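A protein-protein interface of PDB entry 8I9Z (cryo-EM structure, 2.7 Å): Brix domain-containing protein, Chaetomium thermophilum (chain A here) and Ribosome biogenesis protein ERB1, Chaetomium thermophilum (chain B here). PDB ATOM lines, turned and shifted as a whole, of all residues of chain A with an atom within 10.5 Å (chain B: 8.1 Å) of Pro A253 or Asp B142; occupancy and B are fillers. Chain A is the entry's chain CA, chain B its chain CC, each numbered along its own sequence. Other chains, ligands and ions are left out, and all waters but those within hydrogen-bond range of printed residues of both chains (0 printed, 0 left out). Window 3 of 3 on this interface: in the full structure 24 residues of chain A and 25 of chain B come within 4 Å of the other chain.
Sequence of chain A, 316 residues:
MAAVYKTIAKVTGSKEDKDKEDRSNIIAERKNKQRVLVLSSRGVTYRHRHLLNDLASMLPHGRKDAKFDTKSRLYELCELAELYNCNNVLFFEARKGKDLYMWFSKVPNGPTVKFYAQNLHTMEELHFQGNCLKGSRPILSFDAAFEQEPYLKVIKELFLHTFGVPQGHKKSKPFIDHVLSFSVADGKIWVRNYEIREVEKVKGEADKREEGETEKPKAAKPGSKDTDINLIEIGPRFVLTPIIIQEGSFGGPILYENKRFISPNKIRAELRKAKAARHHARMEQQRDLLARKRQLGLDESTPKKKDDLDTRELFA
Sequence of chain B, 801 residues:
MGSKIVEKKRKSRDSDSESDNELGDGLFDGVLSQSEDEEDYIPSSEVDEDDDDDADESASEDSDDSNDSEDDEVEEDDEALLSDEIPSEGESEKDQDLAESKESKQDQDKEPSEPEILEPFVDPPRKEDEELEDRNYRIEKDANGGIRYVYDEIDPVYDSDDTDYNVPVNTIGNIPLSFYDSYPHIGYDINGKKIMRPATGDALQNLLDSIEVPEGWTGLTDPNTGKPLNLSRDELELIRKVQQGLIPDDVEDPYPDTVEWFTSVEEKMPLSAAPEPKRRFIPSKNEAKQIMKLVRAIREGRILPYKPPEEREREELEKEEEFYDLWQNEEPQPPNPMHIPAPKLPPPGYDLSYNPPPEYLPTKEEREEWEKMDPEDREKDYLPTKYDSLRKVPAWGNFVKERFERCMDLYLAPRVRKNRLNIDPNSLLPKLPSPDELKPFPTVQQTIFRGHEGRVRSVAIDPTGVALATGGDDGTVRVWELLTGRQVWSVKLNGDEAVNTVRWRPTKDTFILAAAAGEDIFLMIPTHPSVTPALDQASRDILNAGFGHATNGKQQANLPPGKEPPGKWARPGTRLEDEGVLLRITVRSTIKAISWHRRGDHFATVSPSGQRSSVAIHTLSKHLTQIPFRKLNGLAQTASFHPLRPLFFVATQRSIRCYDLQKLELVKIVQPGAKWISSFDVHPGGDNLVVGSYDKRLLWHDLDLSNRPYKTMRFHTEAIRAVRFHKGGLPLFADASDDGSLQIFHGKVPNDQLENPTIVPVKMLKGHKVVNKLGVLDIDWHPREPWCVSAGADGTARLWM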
ATOM      1  N   TRP A 103      16.404  15.393 -20.017  1.00  0.00           N
ATOM      2  CA  TRP A 103      17.596  14.675 -20.445  1.00  0.00           C
ATOM      3  C   TRP A 103      17.997  13.681 -19.366  1.00  0.00           C
ATOM      4  O   TRP A 103      18.042  14.032 -18.185  1.00  0.00           O
ATOM      5  CB  TRP A 103      18.759  15.631 -20.718  1.00  0.00           C
ATOM      6  CG  TRP A 103      18.540  16.614 -21.820  1.00  0.00           C
ATOM      7  CD1 TRP A 103      17.657  17.653 -21.831  1.00  0.00           C
ATOM      8  CD2 TRP A 103      19.247  16.680 -23.060  1.00  0.00           C
ATOM      9  NE1 TRP A 103      17.758  18.350 -23.008  1.00  0.00           N
ATOM     10  CE2 TRP A 103      18.734  17.775 -23.777  1.00  0.00           C
ATOM     11  CE3 TRP A 103      20.264  15.919 -23.634  1.00  0.00           C
ATOM     12  CZ2 TRP A 103      19.197  18.120 -25.036  1.00  0.00           C
ATOM     13  CZ3 TRP A 103      20.722  16.264 -24.887  1.00  0.00           C
ATOM     14  CH2 TRP A 103      20.192  17.354 -25.573  1.00  0.00           C
ATOM     15  N   ASN A 109      30.772   9.027 -19.723  1.00  0.00           N
ATOM     16  CA  ASN A 109      30.837   8.476 -21.073  1.00  0.00           C
ATOM     17  C   ASN A 109      29.530   7.899 -21.589  1.00  0.00           C
ATOM     18  O   ASN A 109      29.415   7.699 -22.800  1.00  0.00           O
ATOM     19  CB  ASN A 109      31.904   7.376 -21.149  1.00  0.00           C
ATOM     20  CG  ASN A 109      33.246   7.828 -20.637  1.00  0.00           C
ATOM     21  OD1 ASN A 109      33.939   8.604 -21.288  1.00  0.00           O
ATOM     22  ND2 ASN A 109      33.626   7.337 -19.467  1.00  0.00           N
ATOM     23  N   GLY A 110      28.546   7.633 -20.738  1.00  0.00           N
ATOM     24  CA  GLY A 110      27.425   6.801 -21.100  1.00  0.00           C
ATOM     25  C   GLY A 110      26.463   7.443 -22.073  1.00  0.00           C
ATOM     26  O   GLY A 110      26.679   8.555 -22.563  1.00  0.00           O
ATOM     27  N   PRO A 111      25.377   6.740 -22.376  1.00  0.00           N
ATOM     28  CA  PRO A 111      24.389   7.265 -23.319  1.00  0.00           C
ATOM     29  C   PRO A 111      23.615   8.431 -22.725  1.00  0.00           C
ATOM     30  O   PRO A 111      23.644   8.706 -21.526  1.00  0.00           O
ATOM     31  CB  PRO A 111      23.476   6.064 -23.585  1.00  0.00           C
ATOM     32  CG  PRO A 111      24.245   4.885 -23.121  1.00  0.00           C
ATOM     33  CD  PRO A 111      25.048   5.369 -21.968  1.00  0.00           C
ATOM     34  N   THR A 112      22.919   9.132 -23.612  1.00  0.00           N
ATOM     35  CA  THR A 112      22.124  10.295 -23.255  1.00  0.00           C
ATOM     36  C   THR A 112      20.893  10.317 -24.139  1.00  0.00           C
ATOM     37  O   THR A 112      21.013  10.210 -25.361  1.00  0.00           O
ATOM     38  CB  THR A 112      22.921  11.586 -23.437  1.00  0.00           C
ATOM     39  OG1 THR A 112      24.125  11.511 -22.666  1.00  0.00           O
ATOM     40  CG2 THR A 112      22.108  12.793 -22.998  1.00  0.00           C
ATOM     41  N   VAL A 113      19.723  10.468 -23.532  1.00  0.00           N
ATOM     42  CA  VAL A 113      18.472  10.528 -24.271  1.00  0.00           C
ATOM     43  C   VAL A 113      17.788  11.853 -23.965  1.00  0.00           C
ATOM     44  O   VAL A 113      17.808  12.325 -22.825  1.00  0.00           O
ATOM     45  CB  VAL A 113      17.570   9.313 -23.951  1.00  0.00           C
ATOM     46  CG1 VAL A 113      17.362   9.155 -22.459  1.00  0.00           C
ATOM     47  CG2 VAL A 113      16.252   9.378 -24.703  1.00  0.00           C
ATOM     48  N   ILE A 244      15.964  11.919 -29.327  1.00  0.00           N
ATOM     49  CA  ILE A 244      17.285  11.509 -29.787  1.00  0.00           C
ATOM     50  C   ILE A 244      17.994  10.732 -28.687  1.00  0.00           C
ATOM     51  O   ILE A 244      17.673  10.861 -27.506  1.00  0.00           O
ATOM     52  CB  ILE A 244      18.099  12.741 -30.261  1.00  0.00           C
ATOM     53  CG1 ILE A 244      18.915  12.361 -31.478  1.00  0.00           C
ATOM     54  CG2 ILE A 244      18.987  13.300 -29.159  1.00  0.00           C
ATOM     55  CD1 ILE A 244      19.306  13.497 -32.300  1.00  0.00           C
ATOM     56  N   ILE A 245      18.940   9.885 -29.089  1.00  0.00           N
ATOM     57  CA  ILE A 245      19.811   9.137 -28.187  1.00  0.00           C
ATOM     58  C   ILE A 245      21.245   9.353 -28.651  1.00  0.00           C
ATOM     59  O   ILE A 245      21.579   9.045 -29.800  1.00  0.00           O
ATOM     60  CB  ILE A 245      19.482   7.634 -28.165  1.00  0.00           C
ATOM     61  CG1 ILE A 245      18.048   7.384 -27.697  1.00  0.00           C
ATOM     62  CG2 ILE A 245      20.467   6.901 -27.282  1.00  0.00           C
ATOM     63  CD1 ILE A 245      17.725   5.930 -27.461  1.00  0.00           C
ATOM     64  N   GLN A 246      22.088   9.870 -27.765  1.00  0.00           N
ATOM     65  CA  GLN A 246      23.477  10.175 -28.067  1.00  0.00           C
ATOM     66  C   GLN A 246      24.391   9.104 -27.489  1.00  0.00           C
ATOM     67  O   GLN A 246      24.088   8.476 -26.474  1.00  0.00           O
ATOM     68  CB  GLN A 246      23.867  11.547 -27.506  1.00  0.00           C
ATOM     69  CG  GLN A 246      23.935  12.645 -28.537  1.00  0.00           C
ATOM     70  CD  GLN A 246      23.583  13.999 -27.967  1.00  0.00           C
ATOM     71  OE1 GLN A 246      23.206  14.115 -26.804  1.00  0.00           O
ATOM     72  NE2 GLN A 246      23.703  15.034 -28.788  1.00  0.00           N
ATOM     73  N   GLU A 247      25.525   8.900 -28.150  1.00  0.00           N
ATOM     74  CA  GLU A 247      26.530   7.992 -27.618  1.00  0.00           C
ATOM     75  C   GLU A 247      27.384   8.656 -26.553  1.00  0.00           C
ATOM     76  O   GLU A 247      27.782   7.997 -25.585  1.00  0.00           O
ATOM     77  CB  GLU A 247      27.416   7.457 -28.747  1.00  0.00           C
ATOM     78  CG  GLU A 247      28.414   6.402 -28.298  1.00  0.00           C
ATOM     79  CD  GLU A 247      29.460   6.095 -29.342  1.00  0.00           C
ATOM     80  OE1 GLU A 247      29.690   6.942 -30.222  1.00  0.00           O
ATOM     81  OE2 GLU A 247      30.055   4.999 -29.282  1.00  0.00           O
ATOM     82  N   GLY A 248      27.648   9.956 -26.694  1.00  0.00           N
ATOM     83  CA  GLY A 248      28.413  10.695 -25.717  1.00  0.00           C
ATOM     84  C   GLY A 248      27.564  11.183 -24.562  1.00  0.00           C
ATOM     85  O   GLY A 248      26.385  10.864 -24.431  1.00  0.00           O
ATOM     86  N   SER A 249      28.194  11.991 -23.710  1.00  0.00           N
ATOM     87  CA  SER A 249      27.564  12.391 -22.457  1.00  0.00           C
ATOM     88  C   SER A 249      26.498  13.457 -22.671  1.00  0.00           C
ATOM     89  O   SER A 249      25.379  13.322 -22.167  1.00  0.00           O
ATOM     90  CB  SER A 249      28.623  12.888 -21.480  1.00  0.00           C
ATOM     91  OG  SER A 249      28.052  13.168 -20.215  1.00  0.00           O
ATOM     92  N   PHE A 250      26.827  14.534 -23.367  1.00  0.00           N
ATOM     93  CA  PHE A 250      25.820  15.493 -23.798  1.00  0.00           C
ATOM     94  C   PHE A 250      26.153  15.965 -25.208  1.00  0.00           C
ATOM     95  O   PHE A 250      26.055  17.147 -25.538  1.00  0.00           O
ATOM     96  CB  PHE A 250      25.709  16.654 -22.814  1.00  0.00           C
ATOM     97  CG  PHE A 250      24.747  16.399 -21.703  1.00  0.00           C
ATOM     98  CD1 PHE A 250      23.388  16.485 -21.923  1.00  0.00           C
ATOM     99  CD2 PHE A 250      25.199  16.056 -20.444  1.00  0.00           C
ATOM    100  CE1 PHE A 250      22.496  16.245 -20.905  1.00  0.00           C
ATOM    101  CE2 PHE A 250      24.311  15.811 -19.421  1.00  0.00           C
ATOM    102  CZ  PHE A 250      22.958  15.905 -19.652  1.00  0.00           C
ATOM    103  N   GLY A 251      26.549  15.028 -26.053  1.00  0.00           N
ATOM    104  CA  GLY A 251      27.026  15.336 -27.379  1.00  0.00           C
ATOM    105  C   GLY A 251      27.884  14.205 -27.894  1.00  0.00           C
ATOM    106  O   GLY A 251      28.666  13.624 -27.140  1.00  0.00           O
ATOM    107  N   GLY A 252      27.740  13.877 -29.167  1.00  0.00           N
ATOM    108  CA  GLY A 252      28.414  12.744 -29.742  1.00  0.00           C
ATOM    109  C   GLY A 252      27.626  12.208 -30.914  1.00  0.00           C
ATOM    110  O   GLY A 252      26.715  12.866 -31.420  1.00  0.00           O
ATOM    111  N   PRO A 253      27.971  11.011 -31.376  1.00  0.00           N
ATOM    112  CA  PRO A 253      27.249  10.423 -32.508  1.00  0.00           C
ATOM    113  C   PRO A 253      25.805  10.111 -32.146  1.00  0.00           C
ATOM    114  O   PRO A 253      25.480   9.822 -30.994  1.00  0.00           O
ATOM    115  CB  PRO A 253      28.048   9.154 -32.811  1.00  0.00           C
ATOM    116  CG  PRO A 253      29.393   9.438 -32.273  1.00  0.00           C
ATOM    117  CD  PRO A 253      29.171  10.235 -31.037  1.00  0.00           C
ATOM    118  N   ILE A 254      24.936  10.185 -33.145  1.00  0.00           N
ATOM    119  CA  ILE A 254      23.507   9.987 -32.962  1.00  0.00           C
ATOM    120  C   ILE A 254      23.187   8.538 -33.284  1.00  0.00           C
ATOM    121  O   ILE A 254      23.405   8.079 -34.410  1.00  0.00           O
ATOM    122  CB  ILE A 254      22.695  10.944 -33.846  1.00  0.00           C
ATOM    123  CG1 ILE A 254      23.019  12.391 -33.485  1.00  0.00           C
ATOM    124  CG2 ILE A 254      21.222  10.650 -33.732  1.00  0.00           C
ATOM    125  CD1 ILE A 254      22.827  12.712 -32.037  1.00  0.00           C
ATOM    126  N   LEU A 255      22.675   7.815 -32.295  1.00  0.00           N
ATOM    127  CA  LEU A 255      22.335   6.416 -32.488  1.00  0.00           C
ATOM    128  C   LEU A 255      20.882   6.234 -32.896  1.00  0.00           C
ATOM    129  O   LEU A 255      20.571   5.341 -33.691  1.00  0.00           O
ATOM    130  CB  LEU A 255      22.634   5.632 -31.211  1.00  0.00           C
ATOM    131  CG  LEU A 255      24.067   5.819 -30.715  1.00  0.00           C
ATOM    132  CD1 LEU A 255      24.271   5.116 -29.391  1.00  0.00           C
ATOM    133  CD2 LEU A 255      25.059   5.316 -31.743  1.00  0.00           C
ATOM    134  N   TYR A 256      19.983   7.062 -32.370  1.00  0.00           N
ATOM    135  CA  TYR A 256      18.576   7.004 -32.730  1.00  0.00           C
ATOM    136  C   TYR A 256      18.034   8.413 -32.908  1.00  0.00           C
ATOM    137  O   TYR A 256      18.329   9.300 -32.108  1.00  0.00           O
ATOM    138  CB  TYR A 256      17.750   6.278 -31.667  1.00  0.00           C
ATOM    139  CG  TYR A 256      16.274   6.263 -31.973  1.00  0.00           C
ATOM    140  CD1 TYR A 256      15.775   5.510 -33.024  1.00  0.00           C
ATOM    141  CD2 TYR A 256      15.383   7.017 -31.227  1.00  0.00           C
ATOM    142  CE1 TYR A 256      14.428   5.498 -33.314  1.00  0.00           C
ATOM    143  CE2 TYR A 256      14.038   7.014 -31.512  1.00  0.00           C
ATOM    144  CZ  TYR A 256      13.567   6.252 -32.554  1.00  0.00           C
ATOM    145  OH  TYR A 256      12.224   6.244 -32.841  1.00  0.00           O
ATOM    146  N   GLU A 257      17.237   8.605 -33.956  1.00  0.00           N
ATOM    147  CA  GLU A 257      16.517   9.845 -34.197  1.00  0.00           C
ATOM    148  C   GLU A 257      15.050   9.516 -34.408  1.00  0.00           C
ATOM    149  O   GLU A 257      14.723   8.483 -34.998  1.00  0.00           O
ATOM    150  CB  GLU A 257      17.070  10.591 -35.416  1.00  0.00           C
ATOM    151  CG  GLU A 257      17.250  12.080 -35.203  1.00  0.00           C
ATOM    152  CD  GLU A 257      17.262  12.848 -36.506  1.00  0.00           C
ATOM    153  OE1 GLU A 257      17.512  12.229 -37.560  1.00  0.00           O
ATOM    154  OE2 GLU A 257      17.009  14.070 -36.482  1.00  0.00           O
ATOM    155  N   ILE B 139      41.757   7.521 -26.151  1.00  0.00           N
ATOM    156  CA  ILE B 139      41.231   7.631 -27.505  1.00  0.00           C
ATOM    157  C   ILE B 139      40.753   6.262 -27.959  1.00  0.00           C
ATOM    158  O   ILE B 139      41.534   5.303 -28.005  1.00  0.00           O
ATOM    159  CB  ILE B 139      42.285   8.193 -28.470  1.00  0.00           C
ATOM    160  CG1 ILE B 139      42.561   9.664 -28.163  1.00  0.00           C
ATOM    161  CG2 ILE B 139      41.828   8.024 -29.907  1.00  0.00           C
ATOM    162  CD1 ILE B 139      43.533  10.316 -29.116  1.00  0.00           C
ATOM    163  N   GLU B 140      39.472   6.168 -28.295  1.00  0.00           N
ATOM    164  CA  GLU B 140      38.865   4.964 -28.837  1.00  0.00           C
ATOM    165  C   GLU B 140      38.095   5.340 -30.094  1.00  0.00           C
ATOM    166  O   GLU B 140      38.208   6.459 -30.602  1.00  0.00           O
ATOM    167  CB  GLU B 140      37.947   4.291 -27.810  1.00  0.00           C
ATOM    168  CG  GLU B 140      38.683   3.563 -26.705  1.00  0.00           C
ATOM    169  CD  GLU B 140      37.744   2.808 -25.789  1.00  0.00           C
ATOM    170  OE1 GLU B 140      36.529   2.784 -26.075  1.00  0.00           O
ATOM    171  OE2 GLU B 140      38.217   2.244 -24.781  1.00  0.00           O
ATOM    172  N   LYS B 141      37.304   4.405 -30.606  1.00  0.00           N
ATOM    173  CA  LYS B 141      36.524   4.640 -31.810  1.00  0.00           C
ATOM    174  C   LYS B 141      35.036   4.623 -31.499  1.00  0.00           C
ATOM    175  O   LYS B 141      34.558   3.798 -30.716  1.00  0.00           O
ATOM    176  CB  LYS B 141      36.847   3.614 -32.894  1.00  0.00           C
ATOM    177  CG  LYS B 141      37.842   4.136 -33.916  1.00  0.00           C
ATOM    178  CD  LYS B 141      38.324   3.058 -34.869  1.00  0.00           C
ATOM    179  CE  LYS B 141      37.329   2.789 -35.994  1.00  0.00           C
ATOM    180  NZ  LYS B 141      36.294   1.782 -35.631  1.00  0.00           N
ATOM    181  N   ASP B 142      34.317   5.548 -32.116  1.00  0.00           N
ATOM    182  CA  ASP B 142      32.885   5.693 -31.934  1.00  0.00           C
ATOM    183  C   ASP B 142      32.106   4.886 -32.976  1.00  0.00           C
ATOM    184  O   ASP B 142      32.677   4.166 -33.797  1.00  0.00           O
ATOM    185  CB  ASP B 142      32.565   7.194 -31.858  1.00  0.00           C
ATOM    186  CG  ASP B 142      32.457   7.919 -33.231  1.00  0.00           C
ATOM    187  OD1 ASP B 142      32.351   7.354 -34.341  1.00  0.00           O
ATOM    188  OD2 ASP B 142      32.490   9.164 -33.182  1.00  0.00           O
ATOM    189  N   ALA B 143      30.780   5.041 -32.969  1.00  0.00           N
ATOM    190  CA  ALA B 143      29.923   4.222 -33.820  1.00  0.00           C
ATOM    191  C   ALA B 143      30.022   4.623 -35.286  1.00  0.00           C
ATOM    192  O   ALA B 143      29.739   3.809 -36.172  1.00  0.00           O
ATOM    193  CB  ALA B 143      28.475   4.320 -33.349  1.00  0.00           C
ATOM    194  N   ASN B 144      30.415   5.863 -35.559  1.00  0.00           N
ATOM    195  CA  ASN B 144      30.574   6.355 -36.919  1.00  0.00           C
ATOM    196  C   ASN B 144      32.039   6.427 -37.330  1.00  0.00           C
ATOM    197  O   ASN B 144      32.371   7.080 -38.326  1.00  0.00           O
ATOM    198  CB  ASN B 144      29.907   7.723 -37.057  1.00  0.00           C
ATOM    199  CG  ASN B 144      28.404   7.645 -36.897  1.00  0.00           C
ATOM    200  OD1 ASN B 144      27.834   6.558 -36.843  1.00  0.00           O
ATOM    201  ND2 ASN B 144      27.752   8.797 -36.827  1.00  0.00           N
ATOM    202  N   GLY B 145      32.916   5.763 -36.588  1.00  0.00           N
ATOM    203  CA  GLY B 145      34.337   5.794 -36.874  1.00  0.00           C
ATOM    204  C   GLY B 145      35.006   7.126 -36.619  1.00  0.00           C
ATOM    205  O   GLY B 145      35.852   7.552 -37.415  1.00  0.00           O
ATOM    206  N   GLY B 146      34.648   7.799 -35.527  1.00  0.00           N
ATOM    207  CA  GLY B 146      35.296   9.020 -35.119  1.00  0.00           C
ATOM    208  C   GLY B 146      36.226   8.814 -33.938  1.00  0.00           C
ATOM    209  O   GLY B 146      36.538   7.692 -33.537  1.00  0.00           O
ATOM    210  N   ILE B 147      36.667   9.935 -33.374  1.00  0.00           N
ATOM    211  CA  ILE B 147      37.595   9.920 -32.245  1.00  0.00           C
ATOM    212  C   ILE B 147      36.749  10.024 -30.980  1.00  0.00           C
ATOM    213  O   ILE B 147      36.438  11.115 -30.498  1.00  0.00           O
ATOM    214  CB  ILE B 147      38.634  11.032 -32.340  1.00  0.00           C
ATOM    215  CG1 ILE B 147      39.233  11.079 -33.743  1.00  0.00           C
ATOM    216  CG2 ILE B 147      39.721  10.828 -31.304  1.00  0.00           C
ATOM    217  CD1 ILE B 147      40.272  12.164 -33.925  1.00  0.00           C
ATOM    218  N   ARG B 148      36.377   8.874 -30.430  1.00  0.00           N
ATOM    219  CA  ARG B 148      35.662   8.844 -29.166  1.00  0.00           C
ATOM    220  C   ARG B 148      36.644   8.930 -28.009  1.00  0.00           C
ATOM    221  O   ARG B 148      37.628   8.188 -27.956  1.00  0.00           O
ATOM    222  CB  ARG B 148      34.835   7.567 -29.049  1.00  0.00           C
ATOM    223  CG  ARG B 148      34.280   7.322 -27.665  1.00  0.00           C
ATOM    224  CD  ARG B 148      33.304   6.169 -27.656  1.00  0.00           C
ATOM    225  NE  ARG B 148      32.879   5.835 -26.304  1.00  0.00           N
ATOM    226  CZ  ARG B 148      31.873   6.423 -25.672  1.00  0.00           C
ATOM    227  NH1 ARG B 148      31.162   7.379 -26.246  1.00  0.00           N
ATOM    228  NH2 ARG B 148      31.572   6.041 -24.436  1.00  0.00           N
ATOM    229  N   TYR B 149      36.376   9.837 -27.078  1.00  0.00           N
ATOM    230  CA  TYR B 149      37.206  10.012 -25.897  1.00  0.00           C
ATOM    231  C   TYR B 149      36.512   9.369 -24.707  1.00  0.00           C
ATOM    232  O   TYR B 149      35.333   9.636 -24.453  1.00  0.00           O
ATOM    233  CB  TYR B 149      37.473  11.493 -25.622  1.00  0.00           C
ATOM    234  CG  TYR B 149      38.140  12.213 -26.766  1.00  0.00           C
ATOM    235  CD1 TYR B 149      39.477  11.995 -27.063  1.00  0.00           C
ATOM    236  CD2 TYR B 149      37.436  13.116 -27.545  1.00  0.00           C
ATOM    237  CE1 TYR B 149      40.088  12.648 -28.108  1.00  0.00           C
ATOM    238  CE2 TYR B 149      38.042  13.775 -28.590  1.00  0.00           C
ATOM    239  CZ  TYR B 149      39.366  13.537 -28.869  1.00  0.00           C
ATOM    240  OH  TYR B 149      39.972  14.195 -29.912  1.00  0.00           O
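N of Leu A255 is in hydrogen-bond range of O of Ile A245 (3.0 Å).
O of Pro A253 lies within hydrogen-bond range of N of Glu A247.
The backbone carbonyl oxygen of Arg B148 lies within hydrogen-bond range of the backbone NH of Glu B140, at 2.8 Å.
OD1 of Asp B142 lies within hydrogen-bond range of N of Asn B144 (2.7 Å).
The backbone NH of Gly B145 sits at hydrogen-bond distance from the side-chain carboxylate of Asp B142 (2.8 Å).
OD1 of Asp B142 is in hydrogen-bond range of N of Gly B146 (2.6 Å).
Of chain A, only Glu A247 (3.3 Å) and Pro A253 (3.2 Å) come within 4 Å of Asp B142.
No residue of chain B comes within 4 Å of Gly A252.
No residue of chain A comes within 4 Å of Lys B141.
Of the printed residues of chain A, Ala B143 touches Glu A247 and Leu A255.
No residue of chain A comes within 4 Å of Gly B146.
Of the printed residues of chain A, Tyr B149 touches Asn A109.
Printed residues of chain B within 4 Å of Asn A109: Arg B148 (3.2 Å) and Tyr B149 (3.6 Å).
Of the printed residues of chain A, Arg B148 touches Asn A109 (3.2 Å) and Glu A247 (3.5 Å).
Ile B139 touches none of the printed residues of chain A.
Val A113 touches none of the printed residues of chain B.
The nearest printed residue of chain B that does not touch Glu A247 is Lys B141 (4.9 Å).
Printed residues of chain A that touch a printed residue of chain B: Asn A109, Glu A247, Pro A253 and Leu A255.
Hydrophobic or aromatic side chains of chain A that line the printed part of chain B: Pro A253 and Leu A255.
Along chain A the printed residues that touch a printed residue of chain B span positions 109 to 255.
Of the 11 printed residues of chain B, 4 touch a printed residue of chain A.
Printed residues of chain B that touch a printed residue of chain A: Asp B142, Ala B143, Arg B148 and Tyr B149.
Hydrophobic or aromatic side chains of chain B within 4 Å of the printed part of chain A: Ala B143.
Among the printed residues, 7 pairs touch across the chains.
Among the printed residues, no Asp or Glu carboxylate lies within 4 Å of a Lys or Arg side-chain nitrogen of the other chain.
The guanidinium group (NH2) of Arg B148 lies within hydrogen-bond range of the backbone carbonyl oxygen (O) of Asn A109 (3.2 Å).
NH1 of Arg B148 sits at hydrogen-bond distance from O of Glu A247 (3.5 Å).
Among the printed residues, merely in contact across the chains: Asn A109 with Tyr B149 (3.6 Å), Glu A247 with Asp B142 (3.3 Å), Glu A247 with Ala B143 (3.5 Å), Pro A253 with Asp B142 (3.2 Å) and Leu A255 with Ala B143 (3.9 Å).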
